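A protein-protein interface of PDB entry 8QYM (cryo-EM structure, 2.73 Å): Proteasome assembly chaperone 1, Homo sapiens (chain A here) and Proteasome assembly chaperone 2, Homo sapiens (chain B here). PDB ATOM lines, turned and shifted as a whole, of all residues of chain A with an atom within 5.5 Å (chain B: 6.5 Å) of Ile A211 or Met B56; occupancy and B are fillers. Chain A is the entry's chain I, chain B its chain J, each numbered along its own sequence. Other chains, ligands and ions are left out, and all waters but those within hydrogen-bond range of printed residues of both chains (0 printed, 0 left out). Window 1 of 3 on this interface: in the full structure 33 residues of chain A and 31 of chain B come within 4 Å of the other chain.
O of Val A212 lies within hydrogen-bond range of N of Val B57, 3.0 Å away.
ND2 of Asn B59 lies within hydrogen-bond range of O of Leu A206 (3.2 Å).
The backbone carbonyl oxygen of Ile B74 sits at hydrogen-bond distance from the guanidinium group of Arg B92, at 2.8 Å.
O of Ala A217 is in hydrogen-bond range of OG of Ser A221 (2.7 Å).
Of the printed residues of chain B, Leu A206 touches Asn B59.
Pro A209 touches none of the printed residues of chain B.
Ile A211 touches just these residues of chain B: Met B56 (3.9 Å) and Val B57 (3.5 Å).
Of the printed residues of chain B, Ala A217 touches Met B56 and Val B57.
Of the printed residues of chain B, Ser A221 touches Met B56, Val B57 and Ile B74.
Printed residues of chain A within 4 Å of Pro B55: His A213 (3.5 Å) and Ala A218 (3.8 Å).
Of the printed residues of chain A, Val B57 touches Ile A211, Val A212, Ala A217 and Ser A221.
Ser B93 touches none of the printed residues of chain A.
The nearest residue of chain B that does not touch Ile A211 is Gly B58 (4.8 Å).
Asn B59 touches Gln A208.
CE of Met B56 touches CD1 of Ile A211, 3.9 Å away.
Val B57 touches Ile A211 (O to CB, 3.5 Å).
His A213 touches Pro B55 (CB to O, 3.5 Å).
Ala A217 touches Met B56 (CB to CA, 3.8 Å).
O of Ala A217 touches CG1 of Val B57 (3.7 Å).
Pro B55 touches Ala A218.
OG of Ser A221 touches O of Met B56, at 3.8 Å.
Val B57 touches Ser A221.
OG of Ser A221 touches CG2 of Ile B74, 3.998 Å away.
Of the 12 printed residues of chain B, 5 touch a printed residue of chain A.
Printed residues of chain B that touch a printed residue of chain A: Pro B55, Met B56, Val B57, Asn B59 and Ile B74.
Hydrophobic or aromatic side chains of chain B within 4 Å of the printed part of chain A: Pro B55, Met B56, Val B57 and Ile B74.
Hydrophobic or aromatic side chains of chain A within 4 Å of the printed part of chain B: Ile A211, His A213, Ala A217 and Ala A218.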
ATOM      1  N   LEU A 206     -18.677  21.582 -12.628  1.00  0.00           N
ATOM      2  CA  LEU A 206     -19.171  20.220 -12.782  1.00  0.00           C
ATOM      3  C   LEU A 206     -19.705  19.691 -11.457  1.00  0.00           C
ATOM      4  O   LEU A 206     -19.138  19.951 -10.392  1.00  0.00           O
ATOM      5  CB  LEU A 206     -18.059  19.312 -13.307  1.00  0.00           C
ATOM      6  CG  LEU A 206     -18.460  17.914 -13.781  1.00  0.00           C
ATOM      7  CD1 LEU A 206     -19.568  17.990 -14.811  1.00  0.00           C
ATOM      8  CD2 LEU A 206     -17.260  17.176 -14.345  1.00  0.00           C
ATOM      9  N   GLN A 208     -20.925  16.909  -8.506  1.00  0.00           N
ATOM     10  CA  GLN A 208     -20.030  16.087  -7.702  1.00  0.00           C
ATOM     11  C   GLN A 208     -19.844  14.686  -8.282  1.00  0.00           C
ATOM     12  O   GLN A 208     -18.717  14.346  -8.666  1.00  0.00           O
ATOM     13  CB  GLN A 208     -20.519  16.022  -6.253  1.00  0.00           C
ATOM     14  CG  GLN A 208     -20.521  17.373  -5.554  1.00  0.00           C
ATOM     15  CD  GLN A 208     -19.136  17.974  -5.431  1.00  0.00           C
ATOM     16  OE1 GLN A 208     -18.133  17.265  -5.480  1.00  0.00           O
ATOM     17  NE2 GLN A 208     -19.073  19.290  -5.283  1.00  0.00           N
ATOM     18  N   PRO A 209     -20.887  13.853  -8.405  1.00  0.00           N
ATOM     19  CA  PRO A 209     -20.647  12.449  -8.788  1.00  0.00           C
ATOM     20  C   PRO A 209     -20.041  12.275 -10.173  1.00  0.00           C
ATOM     21  O   PRO A 209     -19.719  11.140 -10.545  1.00  0.00           O
ATOM     22  CB  PRO A 209     -22.044  11.820  -8.715  1.00  0.00           C
ATOM     23  CG  PRO A 209     -22.965  12.941  -8.957  1.00  0.00           C
ATOM     24  CD  PRO A 209     -22.332  14.145  -8.327  1.00  0.00           C
ATOM     25  N   ASN A 210     -19.867  13.348 -10.940  1.00  0.00           N
ATOM     26  CA  ASN A 210     -19.288  13.270 -12.271  1.00  0.00           C
ATOM     27  C   ASN A 210     -17.774  13.421 -12.205  1.00  0.00           C
ATOM     28  O   ASN A 210     -17.252  14.245 -11.450  1.00  0.00           O
ATOM     29  CB  ASN A 210     -19.881  14.349 -13.177  1.00  0.00           C
ATOM     30  CG  ASN A 210     -21.313  14.059 -13.566  1.00  0.00           C
ATOM     31  OD1 ASN A 210     -21.582  13.162 -14.361  1.00  0.00           O
ATOM     32  ND2 ASN A 210     -22.243  14.820 -13.004  1.00  0.00           N
ATOM     33  N   ILE A 211     -17.072  12.616 -13.003  1.00  0.00           N
ATOM     34  CA  ILE A 211     -15.617  12.635 -13.066  1.00  0.00           C
ATOM     35  C   ILE A 211     -15.186  12.678 -14.525  1.00  0.00           C
ATOM     36  O   ILE A 211     -15.951  12.359 -15.436  1.00  0.00           O
ATOM     37  CB  ILE A 211     -14.979  11.419 -12.356  1.00  0.00           C
ATOM     38  CG1 ILE A 211     -15.427  10.118 -13.022  1.00  0.00           C
ATOM     39  CG2 ILE A 211     -15.321  11.415 -10.877  1.00  0.00           C
ATOM     40  CD1 ILE A 211     -14.554   8.935 -12.693  1.00  0.00           C
ATOM     41  N   VAL A 212     -13.936  13.086 -14.736  1.00  0.00           N
ATOM     42  CA  VAL A 212     -13.335  13.171 -16.061  1.00  0.00           C
ATOM     43  C   VAL A 212     -12.019  12.405 -16.040  1.00  0.00           C
ATOM     44  O   VAL A 212     -11.246  12.514 -15.083  1.00  0.00           O
ATOM     45  CB  VAL A 212     -13.100  14.635 -16.490  1.00  0.00           C
ATOM     46  CG1 VAL A 212     -12.647  14.702 -17.938  1.00  0.00           C
ATOM     47  CG2 VAL A 212     -14.357  15.458 -16.285  1.00  0.00           C
ATOM     48  N   HIS A 213     -11.767  11.627 -17.092  1.00  0.00           N
ATOM     49  CA  HIS A 213     -10.516  10.881 -17.180  1.00  0.00           C
ATOM     50  C   HIS A 213      -9.793  11.155 -18.495  1.00  0.00           C
ATOM     51  O   HIS A 213     -10.180  12.056 -19.245  1.00  0.00           O
ATOM     52  CB  HIS A 213     -10.772   9.382 -16.999  1.00  0.00           C
ATOM     53  CG  HIS A 213     -11.551   8.753 -18.111  1.00  0.00           C
ATOM     54  ND1 HIS A 213     -12.840   9.126 -18.423  1.00  0.00           N
ATOM     55  CD2 HIS A 213     -11.228   7.762 -18.975  1.00  0.00           C
ATOM     56  CE1 HIS A 213     -13.274   8.399 -19.438  1.00  0.00           C
ATOM     57  NE2 HIS A 213     -12.315   7.563 -19.791  1.00  0.00           N
ATOM     58  N   ALA A 217      -7.724  15.092 -18.004  1.00  0.00           N
ATOM     59  CA  ALA A 217      -7.567  14.810 -16.584  1.00  0.00           C
ATOM     60  C   ALA A 217      -6.097  14.760 -16.194  1.00  0.00           C
ATOM     61  O   ALA A 217      -5.718  15.245 -15.124  1.00  0.00           O
ATOM     62  CB  ALA A 217      -8.259  13.498 -16.229  1.00  0.00           C
ATOM     63  N   ALA A 218      -5.256  14.177 -17.050  1.00  0.00           N
ATOM     64  CA  ALA A 218      -3.825  14.127 -16.766  1.00  0.00           C
ATOM     65  C   ALA A 218      -3.222  15.525 -16.704  1.00  0.00           C
ATOM     66  O   ALA A 218      -2.439  15.832 -15.796  1.00  0.00           O
ATOM     67  CB  ALA A 218      -3.111  13.282 -17.819  1.00  0.00           C
ATOM     68  N   SER A 221      -4.435  17.275 -13.554  1.00  0.00           N
ATOM     69  CA  SER A 221      -3.768  16.713 -12.385  1.00  0.00           C
ATOM     70  C   SER A 221      -2.342  17.227 -12.265  1.00  0.00           C
ATOM     71  O   SER A 221      -1.885  17.557 -11.164  1.00  0.00           O
ATOM     72  CB  SER A 221      -3.781  15.187 -12.460  1.00  0.00           C
ATOM     73  OG  SER A 221      -5.102  14.692 -12.560  1.00  0.00           O
ATOM     74  N   TYR A 236     -20.940  18.902 -23.257  1.00  0.00           N
ATOM     75  CA  TYR A 236     -21.720  17.669 -23.293  1.00  0.00           C
ATOM     76  C   TYR A 236     -22.728  17.782 -24.429  1.00  0.00           C
ATOM     77  O   TYR A 236     -23.718  18.509 -24.318  1.00  0.00           O
ATOM     78  CB  TYR A 236     -22.417  17.429 -21.957  1.00  0.00           C
ATOM     79  CG  TYR A 236     -21.498  16.914 -20.874  1.00  0.00           C
ATOM     80  CD1 TYR A 236     -21.235  15.559 -20.747  1.00  0.00           C
ATOM     81  CD2 TYR A 236     -20.892  17.786 -19.981  1.00  0.00           C
ATOM     82  CE1 TYR A 236     -20.395  15.086 -19.760  1.00  0.00           C
ATOM     83  CE2 TYR A 236     -20.051  17.322 -18.991  1.00  0.00           C
ATOM     84  CZ  TYR A 236     -19.806  15.970 -18.886  1.00  0.00           C
ATOM     85  OH  TYR A 236     -18.970  15.500 -17.902  1.00  0.00           O
ATOM     86  N   LEU B  53      -1.243   4.760 -12.222  1.00  0.00           N
ATOM     87  CA  LEU B  53      -2.698   4.737 -12.208  1.00  0.00           C
ATOM     88  C   LEU B  53      -3.249   5.621 -13.319  1.00  0.00           C
ATOM     89  O   LEU B  53      -2.625   6.608 -13.716  1.00  0.00           O
ATOM     90  CB  LEU B  53      -3.246   5.208 -10.855  1.00  0.00           C
ATOM     91  CG  LEU B  53      -3.019   4.293  -9.651  1.00  0.00           C
ATOM     92  CD1 LEU B  53      -2.818   5.114  -8.390  1.00  0.00           C
ATOM     93  CD2 LEU B  53      -4.181   3.335  -9.482  1.00  0.00           C
ATOM     94  N   VAL B  54      -4.423   5.252 -13.814  1.00  0.00           N
ATOM     95  CA  VAL B  54      -5.088   6.038 -14.860  1.00  0.00           C
ATOM     96  C   VAL B  54      -5.494   7.393 -14.287  1.00  0.00           C
ATOM     97  O   VAL B  54      -6.075   7.446 -13.188  1.00  0.00           O
ATOM     98  CB  VAL B  54      -6.302   5.281 -15.399  1.00  0.00           C
ATOM     99  CG1 VAL B  54      -6.918   6.022 -16.572  1.00  0.00           C
ATOM    100  CG2 VAL B  54      -5.906   3.873 -15.807  1.00  0.00           C
ATOM    101  N   PRO B  55      -5.206   8.500 -14.967  1.00  0.00           N
ATOM    102  CA  PRO B  55      -5.548   9.815 -14.414  1.00  0.00           C
ATOM    103  C   PRO B  55      -7.051  10.048 -14.370  1.00  0.00           C
ATOM    104  O   PRO B  55      -7.808   9.559 -15.210  1.00  0.00           O
ATOM    105  CB  PRO B  55      -4.866  10.796 -15.377  1.00  0.00           C
ATOM    106  CG  PRO B  55      -3.876   9.980 -16.142  1.00  0.00           C
ATOM    107  CD  PRO B  55      -4.453   8.610 -16.226  1.00  0.00           C
ATOM    108  N   MET B  56      -7.472  10.818 -13.369  1.00  0.00           N
ATOM    109  CA  MET B  56      -8.865  11.216 -13.222  1.00  0.00           C
ATOM    110  C   MET B  56      -8.932  12.420 -12.295  1.00  0.00           C
ATOM    111  O   MET B  56      -8.077  12.595 -11.426  1.00  0.00           O
ATOM    112  CB  MET B  56      -9.728  10.062 -12.692  1.00  0.00           C
ATOM    113  CG  MET B  56      -9.448   9.647 -11.252  1.00  0.00           C
ATOM    114  SD  MET B  56     -10.374  10.574 -10.011  1.00  0.00           S
ATOM    115  CE  MET B  56     -11.889   9.625  -9.937  1.00  0.00           C
ATOM    116  N   VAL B  57      -9.958  13.250 -12.493  1.00  0.00           N
ATOM    117  CA  VAL B  57     -10.171  14.441 -11.679  1.00  0.00           C
ATOM    118  C   VAL B  57     -11.645  14.554 -11.317  1.00  0.00           C
ATOM    119  O   VAL B  57     -12.514  13.935 -11.933  1.00  0.00           O
ATOM    120  CB  VAL B  57      -9.701  15.736 -12.382  1.00  0.00           C
ATOM    121  CG1 VAL B  57      -8.188  15.775 -12.470  1.00  0.00           C
ATOM    122  CG2 VAL B  57     -10.322  15.846 -13.763  1.00  0.00           C
ATOM    123  N   GLY B  58     -11.913  15.360 -10.300  1.00  0.00           N
ATOM    124  CA  GLY B  58     -13.273  15.606  -9.857  1.00  0.00           C
ATOM    125  C   GLY B  58     -13.257  16.576  -8.698  1.00  0.00           C
ATOM    126  O   GLY B  58     -12.200  16.923  -8.162  1.00  0.00           O
ATOM    127  N   ASN B  59     -14.452  17.011  -8.315  1.00  0.00           N
ATOM    128  CA  ASN B  59     -14.598  17.950  -7.210  1.00  0.00           C
ATOM    129  C   ASN B  59     -14.517  17.188  -5.887  1.00  0.00           C
ATOM    130  O   ASN B  59     -14.220  15.992  -5.847  1.00  0.00           O
ATOM    131  CB  ASN B  59     -15.893  18.740  -7.354  1.00  0.00           C
ATOM    132  CG  ASN B  59     -15.670  20.114  -7.955  1.00  0.00           C
ATOM    133  OD1 ASN B  59     -14.554  20.630  -7.954  1.00  0.00           O
ATOM    134  ND2 ASN B  59     -16.735  20.713  -8.473  1.00  0.00           N
ATOM    135  N   SER B  73      -9.873  17.319  -6.859  1.00  0.00           N
ATOM    136  CA  SER B  73      -9.290  16.099  -6.322  1.00  0.00           C
ATOM    137  C   SER B  73      -8.700  15.270  -7.455  1.00  0.00           C
ATOM    138  O   SER B  73      -9.105  15.386  -8.613  1.00  0.00           O
ATOM    139  CB  SER B  73     -10.329  15.271  -5.553  1.00  0.00           C
ATOM    140  OG  SER B  73     -10.677  15.896  -4.331  1.00  0.00           O
ATOM    141  N   ILE B  74      -7.734  14.423  -7.104  1.00  0.00           N
ATOM    142  CA  ILE B  74      -7.046  13.554  -8.045  1.00  0.00           C
ATOM    143  C   ILE B  74      -7.128  12.118  -7.533  1.00  0.00           C
ATOM    144  O   ILE B  74      -7.773  11.834  -6.525  1.00  0.00           O
ATOM    145  CB  ILE B  74      -5.581  13.982  -8.281  1.00  0.00           C
ATOM    146  CG1 ILE B  74      -4.724  13.701  -7.047  1.00  0.00           C
ATOM    147  CG2 ILE B  74      -5.505  15.453  -8.656  1.00  0.00           C
ATOM    148  CD1 ILE B  74      -3.245  13.624  -7.346  1.00  0.00           C
ATOM    149  N   ASN B  75      -6.467  11.205  -8.247  1.00  0.00           N
ATOM    150  CA  ASN B  75      -6.641   9.776  -8.015  1.00  0.00           C
ATOM    151  C   ASN B  75      -5.823   9.235  -6.847  1.00  0.00           C
ATOM    152  O   ASN B  75      -5.929   8.040  -6.551  1.00  0.00           O
ATOM    153  CB  ASN B  75      -6.295   8.993  -9.285  1.00  0.00           C
ATOM    154  CG  ASN B  75      -4.894   9.277  -9.788  1.00  0.00           C
ATOM    155  OD1 ASN B  75      -4.156  10.064  -9.199  1.00  0.00           O
ATOM    156  ND2 ASN B  75      -4.519   8.630 -10.884  1.00  0.00           N
ATOM    157  N   ARG B  92      -8.357   6.079  -6.190  1.00  0.00           N
ATOM    158  CA  ARG B  92      -9.643   6.218  -6.866  1.00  0.00           C
ATOM    159  C   ARG B  92      -9.582   5.819  -8.336  1.00  0.00           C
ATOM    160  O   ARG B  92     -10.385   6.308  -9.134  1.00  0.00           O
ATOM    161  CB  ARG B  92     -10.155   7.655  -6.747  1.00  0.00           C
ATOM    162  CG  ARG B  92     -10.235   8.183  -5.332  1.00  0.00           C
ATOM    163  CD  ARG B  92     -11.188   9.361  -5.251  1.00  0.00           C
ATOM    164  NE  ARG B  92     -11.204   9.960  -3.923  1.00  0.00           N
ATOM    165  CZ  ARG B  92     -10.305  10.831  -3.484  1.00  0.00           C
ATOM    166  NH1 ARG B  92      -9.297  11.226  -4.243  1.00  0.00           N
ATOM    167  NH2 ARG B  92     -10.421  11.316  -2.252  1.00  0.00           N
ATOM    168  N   SER B  93      -8.659   4.945  -8.717  1.00  0.00           N
ATOM    169  CA  SER B  93      -8.493   4.610 -10.126  1.00  0.00           C
ATOM    170  C   SER B  93      -8.021   3.163 -10.231  1.00  0.00           C
ATOM    171  O   SER B  93      -8.103   2.399  -9.266  1.00  0.00           O
ATOM    172  CB  SER B  93      -7.532   5.604 -10.800  1.00  0.00           C
ATOM    173  OG  SER B  93      -7.693   5.592 -12.206  1.00  0.00           O
